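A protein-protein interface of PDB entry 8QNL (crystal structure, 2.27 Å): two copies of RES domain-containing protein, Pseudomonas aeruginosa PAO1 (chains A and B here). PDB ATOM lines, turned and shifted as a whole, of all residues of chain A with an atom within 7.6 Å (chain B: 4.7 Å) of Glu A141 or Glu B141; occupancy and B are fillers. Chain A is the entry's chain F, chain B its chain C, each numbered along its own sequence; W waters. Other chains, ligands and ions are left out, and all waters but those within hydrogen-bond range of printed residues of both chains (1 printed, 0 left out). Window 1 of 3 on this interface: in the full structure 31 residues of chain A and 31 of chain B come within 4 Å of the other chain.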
ATOM      1  N   VAL A  38      24.488 -16.459 -22.808  1.00  0.00           N
ATOM      2  CA  VAL A  38      25.764 -16.386 -23.505  1.00  0.00           C
ATOM      3  C   VAL A  38      25.908 -15.000 -24.120  1.00  0.00           C
ATOM      4  O   VAL A  38      24.946 -14.239 -24.228  1.00  0.00           O
ATOM      5  CB  VAL A  38      25.901 -17.474 -24.592  1.00  0.00           C
ATOM      6  CG1 VAL A  38      25.713 -18.866 -23.995  1.00  0.00           C
ATOM      7  CG2 VAL A  38      24.910 -17.224 -25.720  1.00  0.00           C
ATOM      8  N   GLU A  39      27.131 -14.680 -24.529  1.00  0.00           N
ATOM      9  CA  GLU A  39      27.400 -13.414 -25.187  1.00  0.00           C
ATOM     10  C   GLU A  39      27.162 -13.532 -26.686  1.00  0.00           C
ATOM     11  O   GLU A  39      27.281 -14.605 -27.280  1.00  0.00           O
ATOM     12  CB  GLU A  39      28.835 -12.951 -24.937  1.00  0.00           C
ATOM     13  CG  GLU A  39      29.149 -12.620 -23.492  1.00  0.00           C
ATOM     14  CD  GLU A  39      29.455 -13.852 -22.664  1.00  0.00           C
ATOM     15  OE1 GLU A  39      29.494 -14.965 -23.234  1.00  0.00           O
ATOM     16  OE2 GLU A  39      29.660 -13.708 -21.441  1.00  0.00           O
ATOM     17  N   SER A  40      26.798 -12.407 -27.293  1.00  0.00           N
ATOM     18  CA  SER A  40      26.783 -12.233 -28.735  1.00  0.00           C
ATOM     19  C   SER A  40      27.883 -11.236 -29.101  1.00  0.00           C
ATOM     20  O   SER A  40      28.865 -11.104 -28.349  1.00  0.00           O
ATOM     21  CB  SER A  40      25.373 -11.818 -29.172  1.00  0.00           C
ATOM     22  OG  SER A  40      24.858 -10.792 -28.343  1.00  0.00           O
ATOM     23  N   GLN A  41      27.731 -10.552 -30.235  1.00  0.00           N
ATOM     24  CA  GLN A  41      28.645  -9.514 -30.702  1.00  0.00           C
ATOM     25  C   GLN A  41      30.020 -10.040 -31.107  1.00  0.00           C
ATOM     26  O   GLN A  41      30.865  -9.244 -31.528  1.00  0.00           O
ATOM     27  CB  GLN A  41      28.837  -8.392 -29.670  1.00  0.00           C
ATOM     28  CG  GLN A  41      27.550  -7.696 -29.247  1.00  0.00           C
ATOM     29  CD  GLN A  41      27.797  -6.620 -28.199  1.00  0.00           C
ATOM     30  OE1 GLN A  41      28.131  -6.918 -27.049  1.00  0.00           O
ATOM     31  NE2 GLN A  41      27.626  -5.362 -28.593  1.00  0.00           N
ATOM     32  N   GLU A  42      30.283 -11.342 -30.987  1.00  0.00           N
ATOM     33  CA  GLU A  42      31.534 -11.892 -31.507  1.00  0.00           C
ATOM     34  C   GLU A  42      31.636 -11.705 -33.016  1.00  0.00           C
ATOM     35  O   GLU A  42      32.693 -11.319 -33.528  1.00  0.00           O
ATOM     36  CB  GLU A  42      31.666 -13.378 -31.155  1.00  0.00           C
ATOM     37  CG  GLU A  42      32.014 -13.646 -29.710  1.00  0.00           C
ATOM     38  CD  GLU A  42      30.795 -13.977 -28.880  1.00  0.00           C
ATOM     39  OE1 GLU A  42      29.668 -13.801 -29.395  1.00  0.00           O
ATOM     40  OE2 GLU A  42      30.964 -14.418 -27.722  1.00  0.00           O
ATOM     41  N   VAL A  44      29.884  -9.487 -34.777  1.00  0.00           N
ATOM     42  CA  VAL A  44      29.947  -8.044 -34.977  1.00  0.00           C
ATOM     43  C   VAL A  44      31.373  -7.549 -34.797  1.00  0.00           C
ATOM     44  O   VAL A  44      31.824  -6.653 -35.520  1.00  0.00           O
ATOM     45  CB  VAL A  44      28.970  -7.337 -34.015  1.00  0.00           C
ATOM     46  CG1 VAL A  44      29.078  -5.827 -34.150  1.00  0.00           C
ATOM     47  CG2 VAL A  44      27.546  -7.798 -34.276  1.00  0.00           C
ATOM     48  N   LEU A  47      33.417  -8.142 -37.900  1.00  0.00           N
ATOM     49  CA  LEU A  47      32.931  -7.325 -39.006  1.00  0.00           C
ATOM     50  C   LEU A  47      33.542  -5.926 -38.980  1.00  0.00           C
ATOM     51  O   LEU A  47      33.664  -5.288 -40.032  1.00  0.00           O
ATOM     52  CB  LEU A  47      31.401  -7.258 -38.975  1.00  0.00           C
ATOM     53  CG  LEU A  47      30.733  -6.585 -40.178  1.00  0.00           C
ATOM     54  CD1 LEU A  47      31.254  -7.163 -41.490  1.00  0.00           C
ATOM     55  CD2 LEU A  47      29.216  -6.711 -40.106  1.00  0.00           C
ATOM     56  N   GLN A  48      33.946  -5.440 -37.798  1.00  0.00           N
ATOM     57  CA  GLN A  48      34.633  -4.154 -37.702  1.00  0.00           C
ATOM     58  C   GLN A  48      36.043  -4.197 -38.280  1.00  0.00           C
ATOM     59  O   GLN A  48      36.581  -3.143 -38.644  1.00  0.00           O
ATOM     60  CB  GLN A  48      34.704  -3.691 -36.238  1.00  0.00           C
ATOM     61  CG  GLN A  48      33.384  -3.743 -35.480  1.00  0.00           C
ATOM     62  CD  GLN A  48      32.297  -2.933 -36.151  1.00  0.00           C
ATOM     63  OE1 GLN A  48      31.175  -3.409 -36.327  1.00  0.00           O
ATOM     64  NE2 GLN A  48      32.621  -1.704 -36.533  1.00  0.00           N
ATOM     65  N   ARG A 122      30.151 -11.564 -14.562  1.00  0.00           N
ATOM     66  CA  ARG A 122      30.380 -10.175 -14.943  1.00  0.00           C
ATOM     67  C   ARG A 122      31.194  -9.452 -13.873  1.00  0.00           C
ATOM     68  O   ARG A 122      32.115  -8.689 -14.195  1.00  0.00           O
ATOM     69  CB  ARG A 122      29.049  -9.463 -15.193  1.00  0.00           C
ATOM     70  CG  ARG A 122      28.226 -10.041 -16.347  1.00  0.00           C
ATOM     71  CD  ARG A 122      28.951  -9.923 -17.684  1.00  0.00           C
ATOM     72  NE  ARG A 122      29.203  -8.534 -18.053  1.00  0.00           N
ATOM     73  CZ  ARG A 122      30.007  -8.160 -19.043  1.00  0.00           C
ATOM     74  NH1 ARG A 122      30.639  -9.070 -19.768  1.00  0.00           N
ATOM     75  NH2 ARG A 122      30.179  -6.872 -19.310  1.00  0.00           N
ATOM     76  N   ILE A 138      29.584  -0.930 -18.303  1.00  0.00           N
ATOM     77  CA  ILE A 138      29.779  -1.734 -19.503  1.00  0.00           C
ATOM     78  C   ILE A 138      28.410  -2.137 -20.032  1.00  0.00           C
ATOM     79  O   ILE A 138      27.644  -2.817 -19.339  1.00  0.00           O
ATOM     80  CB  ILE A 138      30.647  -2.967 -19.221  1.00  0.00           C
ATOM     81  CG1 ILE A 138      31.998  -2.540 -18.644  1.00  0.00           C
ATOM     82  CG2 ILE A 138      30.832  -3.785 -20.493  1.00  0.00           C
ATOM     83  CD1 ILE A 138      32.830  -3.690 -18.137  1.00  0.00           C
ATOM     84  N   LEU A 139      28.102  -1.716 -21.257  1.00  0.00           N
ATOM     85  CA  LEU A 139      26.864  -2.090 -21.932  1.00  0.00           C
ATOM     86  C   LEU A 139      27.198  -3.159 -22.966  1.00  0.00           C
ATOM     87  O   LEU A 139      27.853  -2.874 -23.974  1.00  0.00           O
ATOM     88  CB  LEU A 139      26.205  -0.874 -22.583  1.00  0.00           C
ATOM     89  CG  LEU A 139      25.845   0.283 -21.647  1.00  0.00           C
ATOM     90  CD1 LEU A 139      25.202   1.434 -22.413  1.00  0.00           C
ATOM     91  CD2 LEU A 139      24.929  -0.200 -20.532  1.00  0.00           C
ATOM     92  N   SER A 140      26.753  -4.387 -22.712  1.00  0.00           N
ATOM     93  CA  SER A 140      27.003  -5.513 -23.596  1.00  0.00           C
ATOM     94  C   SER A 140      25.682  -6.149 -24.011  1.00  0.00           C
ATOM     95  O   SER A 140      24.630  -5.902 -23.414  1.00  0.00           O
ATOM     96  CB  SER A 140      27.901  -6.562 -22.920  1.00  0.00           C
ATOM     97  OG  SER A 140      27.320  -7.036 -21.717  1.00  0.00           O
ATOM     98  N   GLU A 141      25.752  -6.974 -25.052  1.00  0.00           N
ATOM     99  CA  GLU A 141      24.593  -7.677 -25.584  1.00  0.00           C
ATOM    100  C   GLU A 141      24.767  -9.170 -25.356  1.00  0.00           C
ATOM    101  O   GLU A 141      25.841  -9.724 -25.615  1.00  0.00           O
ATOM    102  CB  GLU A 141      24.400  -7.381 -27.074  1.00  0.00           C
ATOM    103  CG  GLU A 141      24.192  -5.906 -27.376  1.00  0.00           C
ATOM    104  CD  GLU A 141      23.986  -5.624 -28.854  1.00  0.00           C
ATOM    105  OE1 GLU A 141      23.718  -6.575 -29.620  1.00  0.00           O
ATOM    106  OE2 GLU A 141      24.095  -4.443 -29.249  1.00  0.00           O
ATOM    107  N   HIS A 142      23.713  -9.815 -24.871  1.00  0.00           N
ATOM    108  CA  HIS A 142      23.740 -11.229 -24.545  1.00  0.00           C
ATOM    109  C   HIS A 142      22.533 -11.910 -25.167  1.00  0.00           C
ATOM    110  O   HIS A 142      21.595 -11.260 -25.636  1.00  0.00           O
ATOM    111  CB  HIS A 142      23.751 -11.453 -23.027  1.00  0.00           C
ATOM    112  CG  HIS A 142      24.990 -10.959 -22.350  1.00  0.00           C
ATOM    113  ND1 HIS A 142      25.862 -11.800 -21.693  1.00  0.00           N
ATOM    114  CD2 HIS A 142      25.505  -9.714 -22.230  1.00  0.00           C
ATOM    115  CE1 HIS A 142      26.860 -11.092 -21.193  1.00  0.00           C
ATOM    116  NE2 HIS A 142      26.668  -9.823 -21.506  1.00  0.00           N
ATOM    117  N   ALA A 143      22.560 -13.237 -25.157  1.00  0.00           N
ATOM    118  CA  ALA A 143      21.443 -14.025 -25.644  1.00  0.00           C
ATOM    119  C   ALA A 143      21.256 -15.237 -24.747  1.00  0.00           C
ATOM    120  O   ALA A 143      22.232 -15.876 -24.343  1.00  0.00           O
ATOM    121  CB  ALA A 143      21.660 -14.471 -27.098  1.00  0.00           C
ATOM    122  N   PRO A 225      17.398 -12.198 -27.106  1.00  0.00           N
ATOM    123  CA  PRO A 225      18.474 -11.233 -26.861  1.00  0.00           C
ATOM    124  C   PRO A 225      18.248 -10.457 -25.573  1.00  0.00           C
ATOM    125  O   PRO A 225      17.115 -10.193 -25.163  1.00  0.00           O
ATOM    126  CB  PRO A 225      18.406 -10.311 -28.084  1.00  0.00           C
ATOM    127  CG  PRO A 225      16.966 -10.340 -28.474  1.00  0.00           C
ATOM    128  CD  PRO A 225      16.462 -11.733 -28.145  1.00  0.00           C
ATOM    129  N   TRP A 226      19.359 -10.097 -24.930  1.00  0.00           N
ATOM    130  CA  TRP A 226      19.333  -9.376 -23.665  1.00  0.00           C
ATOM    131  C   TRP A 226      20.319  -8.220 -23.705  1.00  0.00           C
ATOM    132  O   TRP A 226      21.400  -8.333 -24.292  1.00  0.00           O
ATOM    133  CB  TRP A 226      19.668 -10.298 -22.478  1.00  0.00           C
ATOM    134  CG  TRP A 226      18.672 -11.390 -22.267  1.00  0.00           C
ATOM    135  CD1 TRP A 226      18.661 -12.611 -22.869  1.00  0.00           C
ATOM    136  CD2 TRP A 226      17.536 -11.361 -21.393  1.00  0.00           C
ATOM    137  NE1 TRP A 226      17.587 -13.346 -22.430  1.00  0.00           N
ATOM    138  CE2 TRP A 226      16.881 -12.602 -21.523  1.00  0.00           C
ATOM    139  CE3 TRP A 226      17.008 -10.407 -20.518  1.00  0.00           C
ATOM    140  CZ2 TRP A 226      15.728 -12.915 -20.806  1.00  0.00           C
ATOM    141  CZ3 TRP A 226      15.864 -10.721 -19.809  1.00  0.00           C
ATOM    142  CH2 TRP A 226      15.237 -11.963 -19.956  1.00  0.00           C
ATOM    143  N   LEU A 227      19.932  -7.107 -23.086  1.00  0.00           N
ATOM    144  CA  LEU A 227      20.831  -5.995 -22.823  1.00  0.00           C
ATOM    145  C   LEU A 227      21.403  -6.155 -21.421  1.00  0.00           C
ATOM    146  O   LEU A 227      20.658  -6.420 -20.473  1.00  0.00           O
ATOM    147  CB  LEU A 227      20.096  -4.658 -22.957  1.00  0.00           C
ATOM    148  CG  LEU A 227      19.493  -4.339 -24.327  1.00  0.00           C
ATOM    149  CD1 LEU A 227      18.859  -2.954 -24.333  1.00  0.00           C
ATOM    150  CD2 LEU A 227      20.551  -4.455 -25.415  1.00  0.00           C
ATOM    151  N   CYS A 228      22.720  -6.006 -21.292  1.00  0.00           N
ATOM    152  CA  CYS A 228      23.404  -6.159 -20.015  1.00  0.00           C
ATOM    153  C   CYS A 228      24.113  -4.867 -19.638  1.00  0.00           C
ATOM    154  O   CYS A 228      24.767  -4.235 -20.475  1.00  0.00           O
ATOM    155  CB  CYS A 228      24.419  -7.303 -20.053  1.00  0.00           C
ATOM    156  SG  CYS A 228      25.279  -7.575 -18.469  1.00  0.00           S
ATOM    157  N   GLU A 229      23.981  -4.488 -18.370  1.00  0.00           N
ATOM    158  CA  GLU A 229      24.620  -3.299 -17.818  1.00  0.00           C
ATOM    159  C   GLU A 229      25.428  -3.732 -16.603  1.00  0.00           C
ATOM    160  O   GLU A 229      24.858  -4.175 -15.601  1.00  0.00           O
ATOM    161  CB  GLU A 229      23.581  -2.242 -17.439  1.00  0.00           C
ATOM    162  CG  GLU A 229      24.154  -1.005 -16.761  1.00  0.00           C
ATOM    163  CD  GLU A 229      23.078  -0.147 -16.114  1.00  0.00           C
ATOM    164  OE1 GLU A 229      21.886  -0.511 -16.208  1.00  0.00           O
ATOM    165  OE2 GLU A 229      23.423   0.889 -15.507  1.00  0.00           O
ATOM    166  N   ALA A 240      16.276  -7.290 -25.103  1.00  0.00           N
ATOM    167  CA  ALA A 240      16.699  -6.352 -26.135  1.00  0.00           C
ATOM    168  C   ALA A 240      15.689  -6.199 -27.267  1.00  0.00           C
ATOM    169  O   ALA A 240      15.839  -5.286 -28.086  1.00  0.00           O
ATOM    170  CB  ALA A 240      18.049  -6.780 -26.722  1.00  0.00           C
ATOM    171  N   GLU B  39      14.131  -5.154 -37.982  1.00  0.00           N
ATOM    172  CA  GLU B  39      15.305  -4.545 -37.375  1.00  0.00           C
ATOM    173  C   GLU B  39      15.288  -4.735 -35.866  1.00  0.00           C
ATOM    174  O   GLU B  39      14.233  -4.810 -35.232  1.00  0.00           O
ATOM    175  CB  GLU B  39      15.394  -3.049 -37.693  1.00  0.00           C
ATOM    176  CG  GLU B  39      15.867  -2.710 -39.098  1.00  0.00           C
ATOM    177  CD  GLU B  39      14.711  -2.543 -40.057  1.00  0.00           C
ATOM    178  OE1 GLU B  39      13.559  -2.598 -39.584  1.00  0.00           O
ATOM    179  OE2 GLU B  39      14.947  -2.355 -41.272  1.00  0.00           O
ATOM    180  N   SER B  40      16.484  -4.844 -35.293  1.00  0.00           N
ATOM    181  CA  SER B  40      16.722  -4.742 -33.865  1.00  0.00           C
ATOM    182  C   SER B  40      17.411  -3.401 -33.600  1.00  0.00           C
ATOM    183  O   SER B  40      17.273  -2.472 -34.417  1.00  0.00           O
ATOM    184  CB  SER B  40      17.508  -5.977 -33.400  1.00  0.00           C
ATOM    185  OG  SER B  40      18.684  -6.178 -34.166  1.00  0.00           O
ATOM    186  N   GLN B  41      18.128  -3.295 -32.482  1.00  0.00           N
ATOM    187  CA  GLN B  41      18.894  -2.110 -32.101  1.00  0.00           C
ATOM    188  C   GLN B  41      18.029  -0.903 -31.740  1.00  0.00           C
ATOM    189  O   GLN B  41      18.582   0.155 -31.425  1.00  0.00           O
ATOM    190  CB  GLN B  41      19.895  -1.677 -33.184  1.00  0.00           C
ATOM    191  CG  GLN B  41      20.931  -2.731 -33.542  1.00  0.00           C
ATOM    192  CD  GLN B  41      21.887  -2.253 -34.626  1.00  0.00           C
ATOM    193  OE1 GLN B  41      21.496  -2.059 -35.783  1.00  0.00           O
ATOM    194  NE2 GLN B  41      23.151  -2.065 -34.259  1.00  0.00           N
ATOM    195  N   VAL B  44      18.754  -0.714 -28.060  1.00  0.00           N
ATOM    196  CA  VAL B  44      20.139  -0.253 -27.973  1.00  0.00           C
ATOM    197  C   VAL B  44      20.220   1.238 -28.256  1.00  0.00           C
ATOM    198  O   VAL B  44      21.000   1.959 -27.621  1.00  0.00           O
ATOM    199  CB  VAL B  44      21.024  -1.067 -28.944  1.00  0.00           C
ATOM    200  CG1 VAL B  44      22.450  -0.527 -28.985  1.00  0.00           C
ATOM    201  CG2 VAL B  44      21.026  -2.533 -28.553  1.00  0.00           C
ATOM    202  N   LEU B 139      26.315  -0.991 -41.792  1.00  0.00           N
ATOM    203  CA  LEU B 139      26.300  -2.241 -41.047  1.00  0.00           C
ATOM    204  C   LEU B 139      25.197  -2.142 -40.000  1.00  0.00           C
ATOM    205  O   LEU B 139      25.318  -1.381 -39.034  1.00  0.00           O
ATOM    206  CB  LEU B 139      27.655  -2.507 -40.396  1.00  0.00           C
ATOM    207  CG  LEU B 139      28.886  -2.471 -41.302  1.00  0.00           C
ATOM    208  CD1 LEU B 139      30.159  -2.680 -40.492  1.00  0.00           C
ATOM    209  CD2 LEU B 139      28.754  -3.528 -42.376  1.00  0.00           C
ATOM    210  N   SER B 140      24.122  -2.898 -40.199  1.00  0.00           N
ATOM    211  CA  SER B 140      22.988  -2.911 -39.291  1.00  0.00           C
ATOM    212  C   SER B 140      22.700  -4.341 -38.860  1.00  0.00           C
ATOM    213  O   SER B 140      23.193  -5.305 -39.454  1.00  0.00           O
ATOM    214  CB  SER B 140      21.741  -2.296 -39.940  1.00  0.00           C
ATOM    215  OG  SER B 140      21.342  -3.052 -41.072  1.00  0.00           O
ATOM    216  N   GLU B 141      21.900  -4.469 -37.809  1.00  0.00           N
ATOM    217  CA  GLU B 141      21.568  -5.763 -37.234  1.00  0.00           C
ATOM    218  C   GLU B 141      20.065  -5.972 -37.318  1.00  0.00           C
ATOM    219  O   GLU B 141      19.287  -5.052 -37.049  1.00  0.00           O
ATOM    220  CB  GLU B 141      22.058  -5.856 -35.788  1.00  0.00           C
ATOM    221  CG  GLU B 141      23.553  -5.613 -35.653  1.00  0.00           C
ATOM    222  CD  GLU B 141      24.046  -5.767 -34.231  1.00  0.00           C
ATOM    223  OE1 GLU B 141      23.400  -6.494 -33.449  1.00  0.00           O
ATOM    224  OE2 GLU B 141      25.082  -5.153 -33.896  1.00  0.00           O
ATOM    225  N   HIS B 142      19.665  -7.175 -37.714  1.00  0.00           N
ATOM    226  CA  HIS B 142      18.268  -7.505 -37.929  1.00  0.00           C
ATOM    227  C   HIS B 142      17.945  -8.805 -37.208  1.00  0.00           C
ATOM    228  O   HIS B 142      18.830  -9.508 -36.714  1.00  0.00           O
ATOM    229  CB  HIS B 142      17.948  -7.630 -39.428  1.00  0.00           C
ATOM    230  CG  HIS B 142      18.123  -6.354 -40.193  1.00  0.00           C
ATOM    231  ND1 HIS B 142      17.079  -5.722 -40.834  1.00  0.00           N
ATOM    232  CD2 HIS B 142      19.221  -5.596 -40.425  1.00  0.00           C
ATOM    233  CE1 HIS B 142      17.526  -4.628 -41.425  1.00  0.00           C
ATOM    234  NE2 HIS B 142      18.823  -4.528 -41.192  1.00  0.00           N
ATOM    235  N   ALA B 143      16.657  -9.125 -37.155  1.00  0.00           N
ATOM    236  CA  ALA B 143      16.193 -10.361 -36.544  1.00  0.00           C
ATOM    237  C   ALA B 143      15.061 -10.934 -37.381  1.00  0.00           C
ATOM    238  O   ALA B 143      14.192 -10.194 -37.847  1.00  0.00           O
ATOM    239  CB  ALA B 143      15.723 -10.134 -35.098  1.00  0.00           C
ATOM    240  N   TRP B 226      20.466 -11.392 -37.412  1.00  0.00           N
ATOM    241  CA  TRP B 226      21.149 -11.310 -38.697  1.00  0.00           C
ATOM    242  C   TRP B 226      21.995 -10.046 -38.758  1.00  0.00           C
ATOM    243  O   TRP B 226      21.610  -9.002 -38.224  1.00  0.00           O
ATOM    244  CB  TRP B 226      20.150 -11.328 -39.875  1.00  0.00           C
ATOM    245  CG  TRP B 226      19.388 -12.618 -40.005  1.00  0.00           C
ATOM    246  CD1 TRP B 226      18.217 -12.944 -39.386  1.00  0.00           C
ATOM    247  CD2 TRP B 226      19.751 -13.755 -40.801  1.00  0.00           C
ATOM    248  NE1 TRP B 226      17.826 -14.212 -39.747  1.00  0.00           N
ATOM    249  CE2 TRP B 226      18.751 -14.731 -40.614  1.00  0.00           C
ATOM    250  CE3 TRP B 226      20.820 -14.041 -41.654  1.00  0.00           C
ATOM    251  CZ2 TRP B 226      18.792 -15.972 -41.246  1.00  0.00           C
ATOM    252  CZ3 TRP B 226      20.858 -15.274 -42.283  1.00  0.00           C
ATOM    253  CH2 TRP B 226      19.851 -16.224 -42.073  1.00  0.00           C
ATOM    254  N   LEU B 227      23.155 -10.148 -39.402  1.00  0.00           N
ATOM    255  CA  LEU B 227      23.974  -8.990 -39.733  1.00  0.00           C
ATOM    256  C   LEU B 227      23.653  -8.573 -41.160  1.00  0.00           C
ATOM    257  O   LEU B 227      23.603  -9.420 -42.056  1.00  0.00           O
ATOM    258  CB  LEU B 227      25.463  -9.311 -39.590  1.00  0.00           C
ATOM    259  CG  LEU B 227      25.933  -9.718 -38.195  1.00  0.00           C
ATOM    260  CD1 LEU B 227      27.441  -9.907 -38.195  1.00  0.00           C
ATOM    261  CD2 LEU B 227      25.518  -8.678 -37.164  1.00  0.00           C
HETATM  262  O   HOH W   1      17.832  -3.437 -29.296  1.00  0.00           O
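The side-chain hydroxyl (OG) of Ser B40 is in hydrogen-bond range of the backbone carbonyl oxygen (O) of Glu B141, at 3.2 Å. The backbone carbonyl oxygen of Val A44 lies close to the side-chain amide oxygen of Gln A48 (3.4 Å). OE1 of Gln A41 sits at hydrogen-bond distance from N of Glu A141 (3.1 Å). N of Glu B141 lies within hydrogen-bond range of OE1 of Gln B41, 3.2 Å away. O of Glu A141 sits at hydrogen-bond distance from OG of Ser A40, 3.1 Å away.
Glu B141 touches Val A44 (OE2 to CG2, 3.6 Å). CG2 of Val A44 touches CD2 of Leu B227, 3.6 Å away. CD2 of Leu A47 touches CD2 of Leu B139 (3.9 Å). Glu A141 touches Val B44. Glu B141 touches Glu A141. Val B44 touches Leu A227 (CG2 to CD2, 3.7 Å).
Val A38 touches none of the printed residues of chain B. Of the printed residues of chain A, Val B44 touches Glu A141 (3.7 Å) and Leu A227 (3.7 Å). Glu B141 touches just these residues of chain A: Val A44 (3.6 Å) and Glu A141 (3.8 Å). Printed residues of chain A within 4 Å of Leu B227: Val A44. The nearest printed residue of chain B that does not touch Glu A141 is Gln B41 (5.6 Å). The nearest printed residue of chain B that does not touch Leu A47 is Leu B227 (4.1 Å).
Of the 11 printed residues of chain B, 4 touch a printed residue of chain A. Printed residues of chain B that touch a printed residue of chain A: Val B44, Leu B139, Glu B141 and Leu B227. Hydrophobic or aromatic side chains of chain B that line the printed part of chain A: Val B44, Leu B139 and Leu B227. Of the 21 printed residues of chain A, 4 touch a printed residue of chain B. Printed residues of chain A that touch a printed residue of chain B: Val A44, Leu A47, Glu A141 and Leu A227. Hydrophobic or aromatic side chains of chain A within 4 Å of the printed part of chain B: Val A44, Leu A47 and Leu A227. Among the printed residues, 6 pairs touch across the chains.
Val A44 touches Glu B141, and with the chains exchanged Glu A141 touches Val B44. Val A44 touches Leu B227, and with the chains exchanged Leu A227 touches Val B44. Glu B141 touches its own counterpart, Glu A141. 11 positions are printed for both chains.
Water W1 lies within hydrogen-bond range of O of Ala A240 (3.0 Å), N of Val B44 (3.1 Å) and N of Gln B41 (3.2 Å).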
